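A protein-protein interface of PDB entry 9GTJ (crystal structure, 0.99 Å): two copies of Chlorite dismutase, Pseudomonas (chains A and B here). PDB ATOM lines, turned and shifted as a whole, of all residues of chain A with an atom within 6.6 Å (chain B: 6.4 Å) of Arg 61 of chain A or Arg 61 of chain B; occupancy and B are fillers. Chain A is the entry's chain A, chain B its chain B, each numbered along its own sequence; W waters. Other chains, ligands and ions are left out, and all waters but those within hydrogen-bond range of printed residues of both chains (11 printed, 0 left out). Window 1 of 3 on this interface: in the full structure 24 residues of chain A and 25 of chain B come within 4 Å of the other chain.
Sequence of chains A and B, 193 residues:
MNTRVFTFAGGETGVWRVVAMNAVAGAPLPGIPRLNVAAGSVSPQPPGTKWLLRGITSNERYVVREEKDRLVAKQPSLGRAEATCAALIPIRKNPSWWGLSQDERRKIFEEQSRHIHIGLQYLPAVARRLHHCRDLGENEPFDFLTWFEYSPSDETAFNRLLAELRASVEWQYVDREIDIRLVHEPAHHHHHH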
ATOM      1  N   ILE A  56     -30.344 -16.615   3.545  1.00  0.00           N
ATOM      2  CA  ILE A  56     -30.648 -17.726   2.644  1.00  0.00           C
ATOM      3  C   ILE A  56     -31.568 -18.708   3.358  1.00  0.00           C
ATOM      4  O   ILE A  56     -31.327 -19.093   4.508  1.00  0.00           O
ATOM      5  CB  ILE A  56     -29.354 -18.367   2.102  1.00  0.00           C
ATOM      6  CG1 ILE A  56     -29.642 -19.256   0.891  1.00  0.00           C
ATOM      7  CG2 ILE A  56     -28.571 -19.122   3.167  1.00  0.00           C
ATOM      8  CD1 ILE A  56     -28.419 -19.812   0.213  1.00  0.00           C
ATOM      9  N   THR A  57     -32.628 -19.144   2.670  1.00  0.00           N
ATOM     10  CA  THR A  57     -33.419 -20.236   3.203  1.00  0.00           C
ATOM     11  C   THR A  57     -32.591 -21.509   3.142  1.00  0.00           C
ATOM     12  O   THR A  57     -31.724 -21.670   2.270  1.00  0.00           O
ATOM     13  CB  THR A  57     -34.774 -20.379   2.507  1.00  0.00           C
ATOM     14  OG1 THR A  57     -34.561 -20.741   1.150  1.00  0.00           O
ATOM     15  CG2 THR A  57     -35.581 -19.106   2.540  1.00  0.00           C
ATOM     16  N   SER A  58     -32.834 -22.451   4.070  1.00  0.00           N
ATOM     17  CA  SER A  58     -31.957 -23.599   4.185  1.00  0.00           C
ATOM     18  C   SER A  58     -32.727 -24.811   4.678  1.00  0.00           C
ATOM     19  O   SER A  58     -33.933 -24.792   4.905  1.00  0.00           O
ATOM     20  CB  SER A  58     -30.763 -23.246   5.062  1.00  0.00           C
ATOM     21  OG  SER A  58     -29.762 -24.253   5.030  1.00  0.00           O
ATOM     22  N   ASN A  59     -31.987 -25.917   4.825  1.00  0.00           N
ATOM     23  CA  ASN A  59     -32.577 -27.143   5.338  1.00  0.00           C
ATOM     24  C   ASN A  59     -32.895 -26.992   6.823  1.00  0.00           C
ATOM     25  O   ASN A  59     -32.305 -26.182   7.552  1.00  0.00           O
ATOM     26  CB  ASN A  59     -31.669 -28.341   5.093  1.00  0.00           C
ATOM     27  CG  ASN A  59     -30.302 -28.161   5.720  1.00  0.00           C
ATOM     28  OD1 ASN A  59     -29.446 -27.480   5.160  1.00  0.00           O
ATOM     29  ND2 ASN A  59     -30.080 -28.795   6.863  1.00  0.00           N
ATOM     30  N   GLU A  60     -33.788 -27.858   7.279  1.00  0.00           N
ATOM     31  CA  GLU A  60     -34.147 -27.927   8.686  1.00  0.00           C
ATOM     32  C   GLU A  60     -32.945 -28.355   9.514  1.00  0.00           C
ATOM     33  O   GLU A  60     -32.172 -29.238   9.135  1.00  0.00           O
ATOM     34  CB  GLU A  60     -35.293 -28.916   8.878  1.00  0.00           C
ATOM     35  CG  GLU A  60     -36.581 -28.377   8.275  1.00  0.00           C
ATOM     36  CD  GLU A  60     -37.534 -29.414   7.735  1.00  0.00           C
ATOM     37  OE1 GLU A  60     -37.094 -30.541   7.453  1.00  0.00           O
ATOM     38  OE2 GLU A  60     -38.702 -29.048   7.545  1.00  0.00           O
ATOM     39  N   ARG A  61     -32.841 -27.726  10.691  1.00  0.00           N
ATOM     40  CA  ARG A  61     -31.772 -27.978  11.631  1.00  0.00           C
ATOM     41  C   ARG A  61     -32.256 -28.696  12.885  1.00  0.00           C
ATOM     42  O   ARG A  61     -31.431 -29.258  13.609  1.00  0.00           O
ATOM     43  CB  ARG A  61     -31.146 -26.638  12.044  1.00  0.00           C
ATOM     44  CG  ARG A  61     -30.730 -25.762  10.875  1.00  0.00           C
ATOM     45  CD  ARG A  61     -29.783 -26.481   9.894  1.00  0.00           C
ATOM     46  NE  ARG A  61     -29.535 -25.672   8.713  1.00  0.00           N
ATOM     47  CZ  ARG A  61     -28.617 -24.704   8.677  1.00  0.00           C
ATOM     48  NH1 ARG A  61     -27.887 -24.461   9.777  1.00  0.00           N
ATOM     49  NH2 ARG A  61     -28.448 -23.895   7.634  1.00  0.00           N
ATOM     50  N   TYR A  62     -33.563 -28.656  13.150  1.00  0.00           N
ATOM     51  CA  TYR A  62     -34.113 -29.158  14.410  1.00  0.00           C
ATOM     52  C   TYR A  62     -35.397 -29.965  14.230  1.00  0.00           C
ATOM     53  O   TYR A  62     -35.614 -30.931  14.962  1.00  0.00           O
ATOM     54  CB  TYR A  62     -34.410 -28.019  15.410  1.00  0.00           C
ATOM     55  CG  TYR A  62     -33.152 -27.280  15.819  1.00  0.00           C
ATOM     56  CD1 TYR A  62     -32.173 -27.901  16.574  1.00  0.00           C
ATOM     57  CD2 TYR A  62     -32.908 -25.984  15.386  1.00  0.00           C
ATOM     58  CE1 TYR A  62     -30.977 -27.260  16.853  1.00  0.00           C
ATOM     59  CE2 TYR A  62     -31.726 -25.330  15.666  1.00  0.00           C
ATOM     60  CZ  TYR A  62     -30.744 -25.970  16.397  1.00  0.00           C
ATOM     61  OH  TYR A  62     -29.548 -25.387  16.678  1.00  0.00           O
ATOM     62  N   VAL A  63     -36.269 -29.566  13.307  1.00  0.00           N
ATOM     63  CA  VAL A  63     -37.595 -30.139  13.283  1.00  0.00           C
ATOM     64  C   VAL A  63     -37.508 -31.618  12.896  1.00  0.00           C
ATOM     65  O   VAL A  63     -36.740 -32.077  12.040  1.00  0.00           O
ATOM     66  CB  VAL A  63     -38.486 -29.281  12.366  1.00  0.00           C
ATOM     67  CG1 VAL A  63     -38.118 -29.449  10.914  1.00  0.00           C
ATOM     68  CG2 VAL A  63     -39.959 -29.558  12.530  1.00  0.00           C
ATOM     69  N   TRP A  98     -23.587 -21.137  19.632  1.00  0.00           N
ATOM     70  CA  TRP A  98     -23.057 -21.765  18.439  1.00  0.00           C
ATOM     71  C   TRP A  98     -22.046 -22.863  18.755  1.00  0.00           C
ATOM     72  O   TRP A  98     -21.811 -23.760  17.934  1.00  0.00           O
ATOM     73  CB  TRP A  98     -22.477 -20.714  17.485  1.00  0.00           C
ATOM     74  CG  TRP A  98     -23.546 -19.797  16.973  1.00  0.00           C
ATOM     75  CD1 TRP A  98     -23.772 -18.495  17.292  1.00  0.00           C
ATOM     76  CD2 TRP A  98     -24.600 -20.179  16.089  1.00  0.00           C
ATOM     77  NE1 TRP A  98     -24.884 -18.042  16.646  1.00  0.00           N
ATOM     78  CE2 TRP A  98     -25.418 -19.056  15.910  1.00  0.00           C
ATOM     79  CE3 TRP A  98     -24.927 -21.367  15.432  1.00  0.00           C
ATOM     80  CZ2 TRP A  98     -26.544 -19.084  15.106  1.00  0.00           C
ATOM     81  CZ3 TRP A  98     -26.040 -21.384  14.621  1.00  0.00           C
ATOM     82  CH2 TRP A  98     -26.834 -20.258  14.456  1.00  0.00           C
ATOM     83  N   GLN A 102     -25.345 -30.558  19.038  1.00  0.00           N
ATOM     84  CA  GLN A 102     -26.667 -30.564  18.427  1.00  0.00           C
ATOM     85  C   GLN A 102     -27.759 -30.954  19.409  1.00  0.00           C
ATOM     86  O   GLN A 102     -28.844 -30.382  19.389  1.00  0.00           O
ATOM     87  CB  GLN A 102     -26.654 -31.497  17.234  1.00  0.00           C
ATOM     88  CG  GLN A 102     -27.993 -31.658  16.533  1.00  0.00           C
ATOM     89  CD  GLN A 102     -28.530 -30.386  15.936  1.00  0.00           C
ATOM     90  OE1 GLN A 102     -27.774 -29.463  15.608  1.00  0.00           O
ATOM     91  NE2 GLN A 102     -29.840 -30.360  15.739  1.00  0.00           N
ATOM     92  N   ARG A 105     -28.605 -27.982  21.742  1.00  0.00           N
ATOM     93  CA  ARG A 105     -29.423 -26.959  21.108  1.00  0.00           C
ATOM     94  C   ARG A 105     -30.838 -27.444  20.848  1.00  0.00           C
ATOM     95  O   ARG A 105     -31.781 -26.679  21.066  1.00  0.00           O
ATOM     96  CB  ARG A 105     -28.750 -26.457  19.833  1.00  0.00           C
ATOM     97  CG  ARG A 105     -27.624 -25.484  20.142  1.00  0.00           C
ATOM     98  CD  ARG A 105     -26.895 -24.940  18.926  1.00  0.00           C
ATOM     99  NE  ARG A 105     -25.826 -25.811  18.437  1.00  0.00           N
ATOM    100  CZ  ARG A 105     -25.931 -26.755  17.506  1.00  0.00           C
ATOM    101  NH1 ARG A 105     -27.009 -26.874  16.742  1.00  0.00           N
ATOM    102  NH2 ARG A 105     -24.925 -27.583  17.341  1.00  0.00           N
ATOM    103  N   ARG A 106     -31.014 -28.685  20.395  1.00  0.00           N
ATOM    104  CA  ARG A 106     -32.383 -29.183  20.196  1.00  0.00           C
ATOM    105  C   ARG A 106     -33.164 -29.175  21.516  1.00  0.00           C
ATOM    106  O   ARG A 106     -34.339 -28.833  21.549  1.00  0.00           O
ATOM    107  CB  ARG A 106     -32.351 -30.592  19.598  1.00  0.00           C
ATOM    108  CG  ARG A 106     -33.678 -31.347  19.619  1.00  0.00           C
ATOM    109  CD  ARG A 106     -34.818 -30.713  18.840  1.00  0.00           C
ATOM    110  NE  ARG A 106     -36.077 -31.366  19.199  1.00  0.00           N
ATOM    111  CZ  ARG A 106     -37.231 -31.311  18.532  1.00  0.00           C
ATOM    112  NH1 ARG A 106     -37.306 -30.815  17.314  1.00  0.00           N
ATOM    113  NH2 ARG A 106     -38.338 -31.772  19.098  1.00  0.00           N
ATOM    114  N   LEU A 130     -37.885 -18.364   7.325  1.00  0.00           N
ATOM    115  CA  LEU A 130     -36.622 -18.308   8.032  1.00  0.00           C
ATOM    116  C   LEU A 130     -35.453 -18.205   7.066  1.00  0.00           C
ATOM    117  O   LEU A 130     -35.337 -19.019   6.143  1.00  0.00           O
ATOM    118  CB  LEU A 130     -36.471 -19.572   8.870  1.00  0.00           C
ATOM    119  CG  LEU A 130     -35.164 -19.760   9.638  1.00  0.00           C
ATOM    120  CD1 LEU A 130     -34.964 -18.655  10.672  1.00  0.00           C
ATOM    121  CD2 LEU A 130     -35.144 -21.141  10.288  1.00  0.00           C
ATOM    122  N   HIS A 132     -31.155 -17.845   6.975  1.00  0.00           N
ATOM    123  CA  HIS A 132     -29.915 -18.030   7.715  1.00  0.00           C
ATOM    124  C   HIS A 132     -28.826 -17.121   7.162  1.00  0.00           C
ATOM    125  O   HIS A 132     -28.640 -17.033   5.943  1.00  0.00           O
ATOM    126  CB  HIS A 132     -29.453 -19.485   7.585  1.00  0.00           C
ATOM    127  CG  HIS A 132     -30.392 -20.484   8.133  1.00  0.00           C
ATOM    128  ND1 HIS A 132     -30.127 -21.160   9.302  1.00  0.00           N
ATOM    129  CD2 HIS A 132     -31.586 -20.908   7.668  1.00  0.00           C
ATOM    130  CE1 HIS A 132     -31.154 -21.954   9.525  1.00  0.00           C
ATOM    131  NE2 HIS A 132     -32.032 -21.846   8.540  1.00  0.00           N
ATOM    132  N   ASP A 135     -23.667 -18.632   7.717  1.00  0.00           N
ATOM    133  CA  ASP A 135     -22.782 -19.331   6.817  1.00  0.00           C
ATOM    134  C   ASP A 135     -22.532 -18.552   5.530  1.00  0.00           C
ATOM    135  O   ASP A 135     -21.840 -19.013   4.646  1.00  0.00           O
ATOM    136  CB  ASP A 135     -23.253 -20.755   6.627  1.00  0.00           C
ATOM    137  CG  ASP A 135     -23.309 -21.527   7.938  1.00  0.00           C
ATOM    138  OD1 ASP A 135     -22.376 -21.435   8.742  1.00  0.00           O
ATOM    139  OD2 ASP A 135     -24.285 -22.253   8.120  1.00  0.00           O
ATOM    140  N   PHE A 144     -29.969 -14.647  11.816  1.00  0.00           N
ATOM    141  CA  PHE A 144     -31.195 -15.032  11.147  1.00  0.00           C
ATOM    142  C   PHE A 144     -31.936 -13.778  10.737  1.00  0.00           C
ATOM    143  O   PHE A 144     -31.929 -12.785  11.449  1.00  0.00           O
ATOM    144  CB  PHE A 144     -32.118 -15.844  12.052  1.00  0.00           C
ATOM    145  CG  PHE A 144     -31.450 -17.042  12.656  1.00  0.00           C
ATOM    146  CD1 PHE A 144     -31.291 -18.203  11.929  1.00  0.00           C
ATOM    147  CD2 PHE A 144     -30.987 -16.993  13.949  1.00  0.00           C
ATOM    148  CE1 PHE A 144     -30.680 -19.301  12.526  1.00  0.00           C
ATOM    149  CE2 PHE A 144     -30.375 -18.083  14.527  1.00  0.00           C
ATOM    150  CZ  PHE A 144     -30.219 -19.238  13.815  1.00  0.00           C
ATOM    151  N   SER B  58     -18.633 -24.555  10.156  1.00  0.00           N
ATOM    152  CA  SER B  58     -19.900 -24.148  10.733  1.00  0.00           C
ATOM    153  C   SER B  58     -20.189 -24.903  12.020  1.00  0.00           C
ATOM    154  O   SER B  58     -19.412 -25.717  12.485  1.00  0.00           O
ATOM    155  CB  SER B  58     -20.983 -24.315   9.691  1.00  0.00           C
ATOM    156  OG  SER B  58     -22.221 -23.743  10.084  1.00  0.00           O
ATOM    157  N   ASN B  59     -21.333 -24.581  12.601  1.00  0.00           N
ATOM    158  CA  ASN B  59     -21.756 -25.262  13.803  1.00  0.00           C
ATOM    159  C   ASN B  59     -22.123 -26.716  13.504  1.00  0.00           C
ATOM    160  O   ASN B  59     -22.457 -27.082  12.384  1.00  0.00           O
ATOM    161  CB  ASN B  59     -22.928 -24.558  14.483  1.00  0.00           C
ATOM    162  CG  ASN B  59     -24.140 -24.466  13.564  1.00  0.00           C
ATOM    163  OD1 ASN B  59     -24.179 -23.621  12.664  1.00  0.00           O
ATOM    164  ND2 ASN B  59     -25.138 -25.304  13.797  1.00  0.00           N
ATOM    165  N   GLU B  60     -22.071 -27.542  14.546  1.00  0.00           N
ATOM    166  CA  GLU B  60     -22.449 -28.941  14.451  1.00  0.00           C
ATOM    167  C   GLU B  60     -23.926 -29.073  14.102  1.00  0.00           C
ATOM    168  O   GLU B  60     -24.767 -28.350  14.632  1.00  0.00           O
ATOM    169  CB  GLU B  60     -22.149 -29.624  15.775  1.00  0.00           C
ATOM    170  CG  GLU B  60     -20.655 -29.782  16.006  1.00  0.00           C
ATOM    171  CD  GLU B  60     -20.239 -29.859  17.457  1.00  0.00           C
ATOM    172  OE1 GLU B  60     -20.991 -29.343  18.317  1.00  0.00           O
ATOM    173  OE2 GLU B  60     -19.113 -30.356  17.739  1.00  0.00           O
ATOM    174  N   ARG B  61     -24.181 -30.014  13.216  1.00  0.00           N
ATOM    175  CA  ARG B  61     -25.519 -30.327  12.745  1.00  0.00           C
ATOM    176  C   ARG B  61     -26.045 -31.643  13.272  1.00  0.00           C
ATOM    177  O   ARG B  61     -27.267 -31.865  13.275  1.00  0.00           O
ATOM    178  CB  ARG B  61     -25.543 -30.366  11.212  1.00  0.00           C
ATOM    179  CG  ARG B  61     -24.903 -29.153  10.560  1.00  0.00           C
ATOM    180  CD  ARG B  61     -25.513 -27.827  10.997  1.00  0.00           C
ATOM    181  NE  ARG B  61     -24.800 -26.688  10.409  1.00  0.00           N
ATOM    182  CZ  ARG B  61     -24.956 -26.296   9.147  1.00  0.00           C
ATOM    183  NH1 ARG B  61     -25.877 -26.857   8.382  1.00  0.00           N
ATOM    184  NH2 ARG B  61     -24.166 -25.356   8.647  1.00  0.00           N
ATOM    185  N   TYR B  62     -25.151 -32.544  13.658  1.00  0.00           N
ATOM    186  CA  TYR B  62     -25.519 -33.903  14.057  1.00  0.00           C
ATOM    187  C   TYR B  62     -24.867 -34.346  15.359  1.00  0.00           C
ATOM    188  O   TYR B  62     -25.473 -35.088  16.135  1.00  0.00           O
ATOM    189  CB  TYR B  62     -25.176 -34.936  12.969  1.00  0.00           C
ATOM    190  CG  TYR B  62     -25.893 -34.652  11.672  1.00  0.00           C
ATOM    191  CD1 TYR B  62     -27.258 -34.800  11.564  1.00  0.00           C
ATOM    192  CD2 TYR B  62     -25.231 -34.191  10.556  1.00  0.00           C
ATOM    193  CE1 TYR B  62     -27.941 -34.493  10.400  1.00  0.00           C
ATOM    194  CE2 TYR B  62     -25.893 -33.860   9.394  1.00  0.00           C
ATOM    195  CZ  TYR B  62     -27.258 -33.997   9.314  1.00  0.00           C
ATOM    196  OH  TYR B  62     -27.959 -33.680   8.188  1.00  0.00           O
ATOM    197  N   VAL B  63     -23.607 -33.974  15.583  1.00  0.00           N
ATOM    198  CA  VAL B  63     -22.845 -34.465  16.725  1.00  0.00           C
ATOM    199  C   VAL B  63     -23.542 -34.160  18.031  1.00  0.00           C
ATOM    200  O   VAL B  63     -23.922 -33.012  18.282  1.00  0.00           O
ATOM    201  CB  VAL B  63     -21.468 -33.732  16.783  1.00  0.00           C
ATOM    202  CG1 VAL B  63     -20.725 -33.828  18.125  1.00  0.00           C
ATOM    203  CG2 VAL B  63     -20.573 -34.164  15.685  1.00  0.00           C
ATOM    204  N   TRP B  98     -31.793 -32.830   1.311  1.00  0.00           N
ATOM    205  CA  TRP B  98     -31.988 -31.554   1.970  1.00  0.00           C
ATOM    206  C   TRP B  98     -33.433 -31.344   2.388  1.00  0.00           C
ATOM    207  O   TRP B  98     -33.687 -30.516   3.234  1.00  0.00           O
ATOM    208  CB  TRP B  98     -31.464 -30.409   1.093  1.00  0.00           C
ATOM    209  CG  TRP B  98     -30.004 -30.553   0.816  1.00  0.00           C
ATOM    210  CD1 TRP B  98     -29.340 -30.812  -0.373  1.00  0.00           C
ATOM    211  CD2 TRP B  98     -28.975 -30.547   1.809  1.00  0.00           C
ATOM    212  NE1 TRP B  98     -27.996 -30.973  -0.144  1.00  0.00           N
ATOM    213  CE2 TRP B  98     -27.747 -30.815   1.176  1.00  0.00           C
ATOM    214  CE3 TRP B  98     -28.959 -30.320   3.185  1.00  0.00           C
ATOM    215  CZ2 TRP B  98     -26.540 -30.840   1.879  1.00  0.00           C
ATOM    216  CZ3 TRP B  98     -27.758 -30.363   3.865  1.00  0.00           C
ATOM    217  CH2 TRP B  98     -26.569 -30.617   3.220  1.00  0.00           C
ATOM    218  N   GLN B 102     -34.826 -33.383  10.320  1.00  0.00           N
ATOM    219  CA  GLN B 102     -33.567 -33.521  11.048  1.00  0.00           C
ATOM    220  C   GLN B 102     -33.380 -34.939  11.584  1.00  0.00           C
ATOM    221  O   GLN B 102     -32.292 -35.503  11.536  1.00  0.00           O
ATOM    222  CB  GLN B 102     -33.502 -32.479  12.162  1.00  0.00           C
ATOM    223  CG  GLN B 102     -32.258 -32.588  12.997  1.00  0.00           C
ATOM    224  CD  GLN B 102     -30.988 -32.311  12.244  1.00  0.00           C
ATOM    225  OE1 GLN B 102     -30.974 -31.633  11.208  1.00  0.00           O
ATOM    226  NE2 GLN B 102     -29.898 -32.809  12.804  1.00  0.00           N
ATOM    227  N   ARG B 105     -32.393 -37.383   8.753  1.00  0.00           N
ATOM    228  CA  ARG B 105     -30.991 -37.294   8.374  1.00  0.00           C
ATOM    229  C   ARG B 105     -30.079 -37.823   9.479  1.00  0.00           C
ATOM    230  O   ARG B 105     -29.096 -38.515   9.166  1.00  0.00           O
ATOM    231  CB  ARG B 105     -30.637 -35.866   7.975  1.00  0.00           C
ATOM    232  CG  ARG B 105     -31.116 -35.550   6.578  1.00  0.00           C
ATOM    233  CD  ARG B 105     -30.821 -34.130   6.089  1.00  0.00           C
ATOM    234  NE  ARG B 105     -31.800 -33.163   6.553  1.00  0.00           N
ATOM    235  CZ  ARG B 105     -31.748 -32.424   7.667  1.00  0.00           C
ATOM    236  NH1 ARG B 105     -30.652 -32.332   8.402  1.00  0.00           N
ATOM    237  NH2 ARG B 105     -32.828 -31.751   8.028  1.00  0.00           N
ATOM    238  N   ARG B 106     -30.346 -37.508  10.744  1.00  0.00           N
ATOM    239  CA  ARG B 106     -29.504 -38.041  11.805  1.00  0.00           C
ATOM    240  C   ARG B 106     -29.525 -39.572  11.791  1.00  0.00           C
ATOM    241  O   ARG B 106     -28.522 -40.227  12.036  1.00  0.00           O
ATOM    242  CB  ARG B 106     -29.959 -37.497  13.159  1.00  0.00           C
ATOM    243  CG  ARG B 106     -29.363 -38.201  14.368  1.00  0.00           C
ATOM    244  CD  ARG B 106     -27.851 -38.058  14.549  1.00  0.00           C
ATOM    245  NE  ARG B 106     -27.401 -38.995  15.551  1.00  0.00           N
ATOM    246  CZ  ARG B 106     -26.234 -38.971  16.186  1.00  0.00           C
ATOM    247  NH1 ARG B 106     -25.397 -37.970  16.063  1.00  0.00           N
ATOM    248  NH2 ARG B 106     -25.894 -39.993  16.936  1.00  0.00           N
ATOM    249  N   HIS B 132     -18.820 -26.342   4.777  1.00  0.00           N
ATOM    250  CA  HIS B 132     -20.174 -26.325   4.223  1.00  0.00           C
ATOM    251  C   HIS B 132     -20.250 -25.306   3.083  1.00  0.00           C
ATOM    252  O   HIS B 132     -19.790 -24.163   3.233  1.00  0.00           O
ATOM    253  CB  HIS B 132     -21.182 -25.908   5.287  1.00  0.00           C
ATOM    254  CG  HIS B 132     -21.275 -26.849   6.437  1.00  0.00           C
ATOM    255  ND1 HIS B 132     -22.369 -27.648   6.628  1.00  0.00           N
ATOM    256  CD2 HIS B 132     -20.427 -27.104   7.459  1.00  0.00           C
ATOM    257  CE1 HIS B 132     -22.197 -28.353   7.721  1.00  0.00           C
ATOM    258  NE2 HIS B 132     -21.034 -28.067   8.249  1.00  0.00           N
ATOM    259  N   ARG B 134     -23.474 -25.017   1.012  1.00  0.00           N
ATOM    260  CA  ARG B 134     -24.798 -24.782   0.434  1.00  0.00           C
ATOM    261  C   ARG B 134     -25.457 -23.501   0.933  1.00  0.00           C
ATOM    262  O   ARG B 134     -26.458 -23.088   0.331  1.00  0.00           O
ATOM    263  CB  ARG B 134     -25.707 -25.975   0.613  1.00  0.00           C
ATOM    264  CG  ARG B 134     -26.471 -26.066   1.901  1.00  0.00           C
ATOM    265  CD  ARG B 134     -27.335 -27.307   1.932  1.00  0.00           C
ATOM    266  NE  ARG B 134     -28.350 -27.315   0.892  1.00  0.00           N
ATOM    267  CZ  ARG B 134     -29.622 -26.911   1.050  1.00  0.00           C
ATOM    268  NH1 ARG B 134     -30.094 -26.624   2.245  1.00  0.00           N
ATOM    269  NH2 ARG B 134     -30.358 -26.805  -0.002  1.00  0.00           N
ATOM    270  N   ASP B 135     -24.944 -22.891   2.003  1.00  0.00           N
ATOM    271  CA  ASP B 135     -25.548 -21.691   2.545  1.00  0.00           C
ATOM    272  C   ASP B 135     -24.649 -20.459   2.422  1.00  0.00           C
ATOM    273  O   ASP B 135     -24.859 -19.453   3.142  1.00  0.00           O
ATOM    274  CB  ASP B 135     -25.947 -21.898   3.991  1.00  0.00           C
ATOM    275  CG  ASP B 135     -26.863 -23.088   4.152  1.00  0.00           C
ATOM    276  OD1 ASP B 135     -27.895 -23.129   3.477  1.00  0.00           O
ATOM    277  OD2 ASP B 135     -26.563 -23.948   4.998  1.00  0.00           O
HETATM  278  O   HOH W   1     -27.774 -25.412  12.583  1.00  0.00           O
HETATM  279  O   HOH W   2     -27.692 -29.098   8.473  1.00  0.00           O
HETATM  280  O   HOH W   3     -23.146 -21.080  11.675  1.00  0.00           O
HETATM  281  O   HOH W   4     -26.898 -26.498   5.698  1.00  0.00           O
HETATM  282  O   HOH W   5     -26.782 -21.521   7.317  1.00  0.00           O
HETATM  283  O   HOH W   6     -26.111 -18.795   5.886  1.00  0.00           O
HETATM  284  O   HOH W   7     -24.071 -24.226   5.934  1.00  0.00           O
HETATM  285  O   HOH W   8     -32.787 -25.762   1.473  1.00  0.00           O
HETATM  286  O   HOH W   9     -34.985 -29.911   5.608  1.00  0.00           O
HETATM  287  O   HOH W  10     -21.483 -26.505  17.228  1.00  0.00           O
HETATM  288  O   HOH W  11     -25.720 -22.770  10.453  1.00  0.00           O
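Water W7 lies within hydrogen-bond range of the side-chain carboxylate (OD2) of Asp 135 of chain B (2.7 Å), the guanidinium group (NH2) of Arg 61 of chain B (2.9 Å) and the side-chain carboxylate (OD2) of Asp 135 of chain A (3.0 Å). Water W1 bridges the side-chain amide nitrogen of Asn 59 of chain B and the guanidinium group of Arg 61 of chain A.
OG of Ser 58 of chain A is in hydrogen-bond range of OD1 of Asp 135 of chain B (2.7 Å). OD1 of Asn 59 of chain A is in hydrogen-bond range of NH1 of Arg 134 of chain B (3.1 Å). OE1 of Gln 102 of chain B sits close to O of Glu 60 of chain A (3.4 Å). The backbone carbonyl oxygen of Glu 60 of chain A sits at hydrogen-bond distance from the guanidinium group of Arg 105 of chain B. The side-chain amide oxygen of Gln 102 of chain B sits close to the backbone carbonyl oxygen of Arg 61 of chain A (3.4 Å). The side-chain carboxylate (OD2) of Asp 135 of chain B lies within salt-bridge range of the guanidinium group (NH2) of Arg 61 of chain A, 3.2 Å away. The backbone NH of Gln 102 of chain B is in hydrogen-bond range of the backbone carbonyl oxygen of Val 63 of chain A (2.9 Å). OE1 of Gln 102 of chain A lies close to O of Glu 60 of chain B (3.4 Å). O of Arg 61 of chain B lies close to OE1 of Gln 102 of chain A, 3.4 Å away. N of Gln 102 of chain A lies within hydrogen-bond range of O of Val 63 of chain B (2.9 Å). O of Glu 60 of chain B is in hydrogen-bond range of NH2 of Arg 105 of chain A, 2.8 Å away. OD1 of Asp 135 of chain A is in hydrogen-bond range of OG of Ser 58 of chain B, 2.7 Å away. The side-chain carboxylate (OD2) of Asp 135 of chain A lies within salt-bridge range of the guanidinium group (NH2) of Arg 61 of chain B. The guanidinium group (NH1) of Arg 61 of chain A lies close to the guanidinium group (NH1) of Arg 61 of chain B (3.4 Å). The backbone carbonyl oxygen (O) of Asp 135 of chain A lies close to the backbone carbonyl oxygen (O) of Asp 135 of chain B (3.4 Å).
Arg 61 of chain A touches just these residues of chain B: Arg 61 (3.4 Å), Gln 102 (3.4 Å) and Asp 135 (3.2 Å). Leu 130 of chain A touches none of the printed residues of chain B. Of the printed residues of chain B, Asp 135 of chain A touches Ser 58 (2.7 Å), Arg 61 (3.1 Å) and Asp 135 (3.4 Å). Of chain A, only Arg 61, Gln 102 and Asp 135 come within 4 Å of Arg 61 of chain B. Printed residues of chain A within 4 Å of Arg 105 of chain B: Asn 59 (3.9 Å) and Glu 60 (2.8 Å). The nearest residue of chain B that does not touch Arg 61 of chain A is Asn 59 of chain B (4.8 Å). The nearest printed residue of chain A that does not touch Arg 61 of chain B is Arg 105 of chain A (4.8 Å). The nearest printed residue of chain A that does not touch Arg 105 of chain B is Arg 61 of chain A (4.8 Å).
Arg 61 of chain A touches Asp 135 of chain B, and with the chains exchanged Asp 135 of chain A touches Arg 61 of chain B. Tyr 62 of chain A touches Gln 102 of chain B, and with the chains exchanged Gln 102 of chain A touches Tyr 62 of chain B.
Among the printed residues, merely in contact across the chains: Ile 56 of chain A with Arg 134 of chain B (3.8 Å), Ile 56 of chain A with Asp 135 of chain B (3.7 Å), Ser 58 of chain A with Arg 134 of chain B (3.7 Å), Asn 59 of chain A with Trp 98 of chain B (3.5 Å), Asn 59 of chain A with Arg 105 of chain B (3.9 Å), Tyr 62 of chain A with Gln 102 of chain B (3.8 Å), Trp 98 of chain A with Asn 59 of chain B (3.5 Å), Gln 102 of chain A with Tyr 62 of chain B (3.9 Å), Gln 102 of chain A with Gln 102 of chain B (3.8 Å) and Arg 105 of chain A with Asn 59 of chain B (3.8 Å).
Hydrophobic or aromatic side chains of chain B within 4 Å of the printed part of chain A: Trp 98. Of the 16 printed residues of chain A, 11 touch a printed residue of chain B. Hydrophobic or aromatic side chains of chain A that line the printed part of chain B: Ile 56 and Trp 98.
O of Ile 56 of chain A sits at hydrogen-bond distance from N of His 132 of chain A (2.8 Å). OG of Ser 58 of chain A is in hydrogen-bond range of OD1 of Asn 59 of chain A, 3.2 Å away. OE1 of Gln 102 of chain B lies within hydrogen-bond range of NH1 of Arg 105 of chain B, 2.9 Å away.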
